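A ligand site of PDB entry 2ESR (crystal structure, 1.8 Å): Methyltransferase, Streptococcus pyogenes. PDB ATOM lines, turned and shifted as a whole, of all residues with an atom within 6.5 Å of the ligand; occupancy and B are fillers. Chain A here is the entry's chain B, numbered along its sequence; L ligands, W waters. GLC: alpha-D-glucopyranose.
An oxygen (O2) of the ligand lies within hydrogen-bond range of the backbone carbonyl oxygen (O) of Gly 32 (2.7 Å). A ring nitrogen (NE2) of His 172 lies within hydrogen-bond range of an oxygen (O6) of the ligand. An oxygen (O3) of the ligand sits at hydrogen-bond distance from the backbone NH of Asn 31 (3.0 Å). O2 of the ligand sits close to O of Asn 31 (3.3 Å). The backbone carbonyl oxygen (O) of Asp 102 sits at hydrogen-bond distance from an oxygen (O6) of the ligand, 3.1 Å away. O of Gln 131 sits at hydrogen-bond distance from O6 of the ligand, at 3.1 Å. NE2 of His 175 is in hydrogen-bond range of O4 of the ligand. The backbone NH of Met 133 sits at hydrogen-bond distance from an oxygen (O6) of the ligand (3.5 Å).
The backbone NH (N) of Gly 32 is in hydrogen-bond range of the backbone carbonyl oxygen (O) of Gly 53. N of His 172 sits at hydrogen-bond distance from OD1 of Asn 169 (3.4 Å). The backbone NH of Met 133 is in hydrogen-bond range of the backbone carbonyl oxygen of Asp 102 (3.1 Å). The side-chain amide nitrogen of Gln 131 lies close to the backbone NH of His 173, at 2.7 Å. The side-chain sulfur (SD) of Met 133 is in hydrogen-bond range of a ring nitrogen (NE2) of His 175 (3.6 Å). A ring nitrogen (NE2) of His 175 lies close to the backbone carbonyl oxygen (O) of Ile 26, at 3.2 Å. The backbone NH (N) of Val 132 sits close to the side-chain amide nitrogen (ND2) of Asn 169 (2.8 Å).
Residues that only touch the ligand: Val 132 (3.5 Å) and Phe 30 (3.6 Å). Hydrophobic or aromatic side chains that line the ligand: Phe 30, Met 133, His 172 and His 175. Nine residues have an atom within 4 Å of the ligand: Phe 30, Asn 31, Gly 32, Asp 102, Gln 131, Val 132, Met 133, His 172 and His 175. The nearest printed residue that does not touch the ligand is Met 54 (4.2 Å).
Water W1 lies within hydrogen-bond range of the side-chain carboxylate of Asp 102, the backbone carbonyl oxygen of Gln 131 and an oxygen (O1) of the ligand.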
ATOM      1  N   ILE A  26     -37.569 -13.524 -24.533  1.00  0.00           N
ATOM      2  CA  ILE A  26     -36.236 -13.944 -24.105  1.00  0.00           C
ATOM      3  C   ILE A  26     -36.153 -15.201 -23.250  1.00  0.00           C
ATOM      4  O   ILE A  26     -35.070 -15.759 -23.073  1.00  0.00           O
ATOM      5  CB  ILE A  26     -35.542 -12.798 -23.330  1.00  0.00           C
ATOM      6  CG1 ILE A  26     -36.230 -12.566 -21.985  1.00  0.00           C
ATOM      7  CG2 ILE A  26     -35.599 -11.514 -24.151  1.00  0.00           C
ATOM      8  CD1 ILE A  26     -35.517 -11.551 -21.099  1.00  0.00           C
ATOM      9  N   TYR A  29     -37.993 -19.347 -19.516  1.00  0.00           N
ATOM     10  CA  TYR A  29     -37.221 -19.728 -18.344  1.00  0.00           C
ATOM     11  C   TYR A  29     -35.723 -19.589 -18.589  1.00  0.00           C
ATOM     12  O   TYR A  29     -35.279 -19.650 -19.727  1.00  0.00           O
ATOM     13  CB  TYR A  29     -37.583 -21.154 -17.927  1.00  0.00           C
ATOM     14  CG  TYR A  29     -39.038 -21.250 -17.528  1.00  0.00           C
ATOM     15  CD1 TYR A  29     -39.480 -20.711 -16.314  1.00  0.00           C
ATOM     16  CD2 TYR A  29     -39.989 -21.794 -18.394  1.00  0.00           C
ATOM     17  CE1 TYR A  29     -40.823 -20.699 -15.976  1.00  0.00           C
ATOM     18  CE2 TYR A  29     -41.345 -21.777 -18.061  1.00  0.00           C
ATOM     19  CZ  TYR A  29     -41.754 -21.230 -16.860  1.00  0.00           C
ATOM     20  OH  TYR A  29     -43.088 -21.191 -16.527  1.00  0.00           O
ATOM     21  N   PHE A  30     -34.956 -19.406 -17.511  1.00  0.00           N
ATOM     22  CA  PHE A  30     -33.513 -19.231 -17.620  1.00  0.00           C
ATOM     23  C   PHE A  30     -32.691 -20.286 -16.876  1.00  0.00           C
ATOM     24  O   PHE A  30     -33.189 -20.977 -15.991  1.00  0.00           O
ATOM     25  CB  PHE A  30     -33.116 -17.840 -17.106  1.00  0.00           C
ATOM     26  CG  PHE A  30     -33.831 -16.718 -17.812  1.00  0.00           C
ATOM     27  CD1 PHE A  30     -33.569 -16.449 -19.143  1.00  0.00           C
ATOM     28  CD2 PHE A  30     -34.762 -15.940 -17.140  1.00  0.00           C
ATOM     29  CE1 PHE A  30     -34.231 -15.414 -19.806  1.00  0.00           C
ATOM     30  CE2 PHE A  30     -35.435 -14.912 -17.783  1.00  0.00           C
ATOM     31  CZ  PHE A  30     -35.167 -14.649 -19.131  1.00  0.00           C
ATOM     32  N   ASN A  31     -31.411 -20.370 -17.225  1.00  0.00           N
ATOM     33  CA  ASN A  31     -30.480 -21.326 -16.638  1.00  0.00           C
ATOM     34  C   ASN A  31     -29.481 -20.739 -15.649  1.00  0.00           C
ATOM     35  O   ASN A  31     -28.355 -21.205 -15.551  1.00  0.00           O
ATOM     36  CB  ASN A  31     -29.703 -22.044 -17.753  1.00  0.00           C
ATOM     37  CG  ASN A  31     -30.580 -22.939 -18.598  1.00  0.00           C
ATOM     38  OD1 ASN A  31     -30.172 -23.373 -19.680  1.00  0.00           O
ATOM     39  ND2 ASN A  31     -31.782 -23.227 -18.123  1.00  0.00           N
ATOM     40  N   GLY A  32     -29.892 -19.710 -14.911  1.00  0.00           N
ATOM     41  CA  GLY A  32     -29.001 -19.089 -13.946  1.00  0.00           C
ATOM     42  C   GLY A  32     -28.137 -17.999 -14.545  1.00  0.00           C
ATOM     43  O   GLY A  32     -28.045 -17.855 -15.763  1.00  0.00           O
ATOM     44  N   GLY A  33     -27.498 -17.204 -13.672  1.00  0.00           N
ATOM     45  CA  GLY A  33     -26.646 -16.131 -14.138  1.00  0.00           C
ATOM     46  C   GLY A  33     -26.908 -14.829 -13.400  1.00  0.00           C
ATOM     47  O   GLY A  33     -27.724 -14.801 -12.474  1.00  0.00           O
ATOM     48  N   GLY A  53     -35.576 -18.142 -13.297  1.00  0.00           N
ATOM     49  CA  GLY A  53     -34.352 -18.891 -13.475  1.00  0.00           C
ATOM     50  C   GLY A  53     -33.005 -18.213 -13.274  1.00  0.00           C
ATOM     51  O   GLY A  53     -31.993 -18.900 -13.148  1.00  0.00           O
ATOM     52  N   MET A  54     -32.971 -16.884 -13.279  1.00  0.00           N
ATOM     53  CA  MET A  54     -31.691 -16.207 -13.089  1.00  0.00           C
ATOM     54  C   MET A  54     -31.272 -16.331 -11.619  1.00  0.00           C
ATOM     55  O   MET A  54     -32.123 -16.459 -10.735  1.00  0.00           O
ATOM     56  CB  MET A  54     -31.800 -14.741 -13.510  1.00  0.00           C
ATOM     57  CG  MET A  54     -32.095 -14.540 -15.017  1.00  0.00           C
ATOM     58  SD  MET A  54     -30.823 -15.394 -16.233  1.00  0.00           S
ATOM     59  CE  MET A  54     -29.250 -14.410 -15.698  1.00  0.00           C
ATOM     60  N   ASP A 102     -24.967 -11.534 -17.426  1.00  0.00           N
ATOM     61  CA  ASP A 102     -25.501 -12.406 -18.470  1.00  0.00           C
ATOM     62  C   ASP A 102     -26.782 -11.868 -19.113  1.00  0.00           C
ATOM     63  O   ASP A 102     -27.084 -12.180 -20.271  1.00  0.00           O
ATOM     64  CB  ASP A 102     -25.761 -13.793 -17.888  1.00  0.00           C
ATOM     65  CG  ASP A 102     -24.540 -14.337 -17.143  1.00  0.00           C
ATOM     66  OD1 ASP A 102     -24.550 -14.345 -15.894  1.00  0.00           O
ATOM     67  OD2 ASP A 102     -23.581 -14.745 -17.819  1.00  0.00           O
ATOM     68  N   LEU A 103     -27.528 -11.074 -18.362  1.00  0.00           N
ATOM     69  CA  LEU A 103     -28.772 -10.487 -18.832  1.00  0.00           C
ATOM     70  C   LEU A 103     -28.827  -9.039 -18.354  1.00  0.00           C
ATOM     71  O   LEU A 103     -28.755  -8.781 -17.158  1.00  0.00           O
ATOM     72  CB  LEU A 103     -29.970 -11.267 -18.285  1.00  0.00           C
ATOM     73  CG  LEU A 103     -31.375 -10.744 -18.625  1.00  0.00           C
ATOM     74  CD1 LEU A 103     -31.545 -10.641 -20.137  1.00  0.00           C
ATOM     75  CD2 LEU A 103     -32.418 -11.711 -18.046  1.00  0.00           C
ATOM     76  N   GLN A 131     -21.718 -14.869 -23.200  1.00  0.00           N
ATOM     77  CA  GLN A 131     -23.075 -15.159 -23.641  1.00  0.00           C
ATOM     78  C   GLN A 131     -23.951 -14.131 -22.949  1.00  0.00           C
ATOM     79  O   GLN A 131     -24.416 -14.363 -21.828  1.00  0.00           O
ATOM     80  CB  GLN A 131     -23.480 -16.569 -23.221  1.00  0.00           C
ATOM     81  CG  GLN A 131     -22.746 -17.657 -23.976  1.00  0.00           C
ATOM     82  CD  GLN A 131     -23.206 -17.764 -25.412  1.00  0.00           C
ATOM     83  OE1 GLN A 131     -22.387 -17.883 -26.331  1.00  0.00           O
ATOM     84  NE2 GLN A 131     -24.511 -17.735 -25.626  1.00  0.00           N
ATOM     85  N   VAL A 132     -24.174 -12.999 -23.593  1.00  0.00           N
ATOM     86  CA  VAL A 132     -24.992 -11.962 -22.994  1.00  0.00           C
ATOM     87  C   VAL A 132     -26.188 -11.582 -23.835  1.00  0.00           C
ATOM     88  O   VAL A 132     -26.177 -11.708 -25.065  1.00  0.00           O
ATOM     89  CB  VAL A 132     -24.156 -10.686 -22.737  1.00  0.00           C
ATOM     90  CG1 VAL A 132     -23.755 -10.062 -24.062  1.00  0.00           C
ATOM     91  CG2 VAL A 132     -24.950  -9.705 -21.893  1.00  0.00           C
ATOM     92  N   MET A 133     -27.220 -11.108 -23.148  1.00  0.00           N
ATOM     93  CA  MET A 133     -28.441 -10.659 -23.788  1.00  0.00           C
ATOM     94  C   MET A 133     -28.766  -9.278 -23.205  1.00  0.00           C
ATOM     95  O   MET A 133     -28.801  -9.101 -21.998  1.00  0.00           O
ATOM     96  CB  MET A 133     -29.545 -11.667 -23.470  1.00  0.00           C
ATOM     97  CG  MET A 133     -30.901 -11.377 -24.030  1.00  0.00           C
ATOM     98  SD  MET A 133     -31.938 -13.030 -23.989  1.00  0.00           S
ATOM     99  CE  MET A 133     -31.757 -13.470 -22.130  1.00  0.00           C
ATOM    100  N   VAL A 168     -27.755  -9.557 -28.702  1.00  0.00           N
ATOM    101  CA  VAL A 168     -27.023 -10.697 -28.182  1.00  0.00           C
ATOM    102  C   VAL A 168     -25.655 -10.744 -28.830  1.00  0.00           C
ATOM    103  O   VAL A 168     -25.444 -10.184 -29.914  1.00  0.00           O
ATOM    104  CB  VAL A 168     -27.750 -12.031 -28.495  1.00  0.00           C
ATOM    105  CG1 VAL A 168     -29.146 -11.994 -27.919  1.00  0.00           C
ATOM    106  CG2 VAL A 168     -27.777 -12.276 -29.997  1.00  0.00           C
ATOM    107  N   ASN A 169     -24.717 -11.399 -28.167  1.00  0.00           N
ATOM    108  CA  ASN A 169     -23.358 -11.506 -28.702  1.00  0.00           C
ATOM    109  C   ASN A 169     -23.340 -12.399 -29.940  1.00  0.00           C
ATOM    110  O   ASN A 169     -24.207 -13.267 -30.111  1.00  0.00           O
ATOM    111  CB  ASN A 169     -22.446 -12.109 -27.636  1.00  0.00           C
ATOM    112  CG  ASN A 169     -22.903 -13.492 -27.208  1.00  0.00           C
ATOM    113  OD1 ASN A 169     -22.344 -14.509 -27.627  1.00  0.00           O
ATOM    114  ND2 ASN A 169     -23.939 -13.539 -26.377  1.00  0.00           N
ATOM    115  N   HIS A 172     -24.187 -16.252 -29.832  1.00  0.00           N
ATOM    116  CA  HIS A 172     -25.015 -16.512 -28.660  1.00  0.00           C
ATOM    117  C   HIS A 172     -25.701 -17.866 -28.876  1.00  0.00           C
ATOM    118  O   HIS A 172     -26.244 -18.099 -29.951  1.00  0.00           O
ATOM    119  CB  HIS A 172     -26.062 -15.404 -28.508  1.00  0.00           C
ATOM    120  CG  HIS A 172     -26.815 -15.457 -27.220  1.00  0.00           C
ATOM    121  ND1 HIS A 172     -27.922 -16.251 -27.032  1.00  0.00           N
ATOM    122  CD2 HIS A 172     -26.608 -14.809 -26.041  1.00  0.00           C
ATOM    123  CE1 HIS A 172     -28.366 -16.096 -25.791  1.00  0.00           C
ATOM    124  NE2 HIS A 172     -27.587 -15.223 -25.180  1.00  0.00           N
ATOM    125  N   HIS A 173     -25.663 -18.728 -27.870  1.00  0.00           N
ATOM    126  CA  HIS A 173     -26.283 -20.049 -27.976  1.00  0.00           C
ATOM    127  C   HIS A 173     -27.804 -19.967 -28.036  1.00  0.00           C
ATOM    128  O   HIS A 173     -28.407 -19.133 -27.369  1.00  0.00           O
ATOM    129  CB  HIS A 173     -25.875 -20.928 -26.787  1.00  0.00           C
ATOM    130  CG  HIS A 173     -24.399 -21.118 -26.654  1.00  0.00           C
ATOM    131  ND1 HIS A 173     -23.589 -21.493 -27.708  1.00  0.00           N
ATOM    132  CD2 HIS A 173     -23.580 -21.008 -25.582  1.00  0.00           C
ATOM    133  CE1 HIS A 173     -22.343 -21.603 -27.293  1.00  0.00           C
ATOM    134  NE2 HIS A 173     -22.305 -21.309 -26.009  1.00  0.00           N
ATOM    135  N   HIS A 174     -28.428 -20.837 -28.826  1.00  0.00           N
ATOM    136  CA  HIS A 174     -29.884 -20.817 -28.933  1.00  0.00           C
ATOM    137  C   HIS A 174     -30.474 -21.088 -27.558  1.00  0.00           C
ATOM    138  O   HIS A 174     -29.812 -21.642 -26.678  1.00  0.00           O
ATOM    139  CB  HIS A 174     -30.355 -21.884 -29.920  1.00  0.00           C
ATOM    140  CG  HIS A 174     -30.322 -23.275 -29.360  1.00  0.00           C
ATOM    141  ND1 HIS A 174     -29.146 -23.981 -29.184  1.00  0.00           N
ATOM    142  CD2 HIS A 174     -31.312 -24.070 -28.903  1.00  0.00           C
ATOM    143  CE1 HIS A 174     -29.428 -25.152 -28.630  1.00  0.00           C
ATOM    144  NE2 HIS A 174     -30.731 -25.228 -28.449  1.00  0.00           N
ATOM    145  N   HIS A 175     -31.733 -20.698 -27.371  1.00  0.00           N
ATOM    146  CA  HIS A 175     -32.410 -20.927 -26.103  1.00  0.00           C
ATOM    147  C   HIS A 175     -33.101 -22.289 -26.121  1.00  0.00           C
ATOM    148  O   HIS A 175     -33.793 -22.624 -27.084  1.00  0.00           O
ATOM    149  CB  HIS A 175     -33.461 -19.839 -25.859  1.00  0.00           C
ATOM    150  CG  HIS A 175     -32.882 -18.519 -25.449  1.00  0.00           C
ATOM    151  ND1 HIS A 175     -31.826 -17.934 -26.095  1.00  0.00           N
ATOM    152  CD2 HIS A 175     -33.243 -17.661 -24.457  1.00  0.00           C
ATOM    153  CE1 HIS A 175     -31.545 -16.772 -25.518  1.00  0.00           C
ATOM    154  NE2 HIS A 175     -32.398 -16.591 -24.530  1.00  0.00           N
HETATM  155  C1  GLC L   1     -27.494 -17.254 -19.201  1.00  0.00           C
HETATM  156  C2  GLC L   1     -28.796 -18.029 -18.876  1.00  0.00           C
HETATM  157  C3  GLC L   1     -29.470 -18.456 -20.189  1.00  0.00           C
HETATM  158  C4  GLC L   1     -29.790 -17.181 -20.996  1.00  0.00           C
HETATM  159  C5  GLC L   1     -28.449 -16.450 -21.274  1.00  0.00           C
HETATM  160  C6  GLC L   1     -28.725 -15.157 -22.060  1.00  0.00           C
HETATM  161  O1  GLC L   1     -26.557 -18.099 -19.896  1.00  0.00           O
HETATM  162  O2  GLC L   1     -28.471 -19.180 -18.093  1.00  0.00           O
HETATM  163  O3  GLC L   1     -30.685 -19.169 -19.897  1.00  0.00           O
HETATM  164  O4  GLC L   1     -30.419 -17.548 -22.224  1.00  0.00           O
HETATM  165  O5  GLC L   1     -27.801 -16.085 -20.017  1.00  0.00           O
HETATM  166  O6  GLC L   1     -27.488 -14.476 -22.314  1.00  0.00           O
HETATM  167  O   HOH W   1     -24.016 -16.164 -19.926  1.00  0.00           O
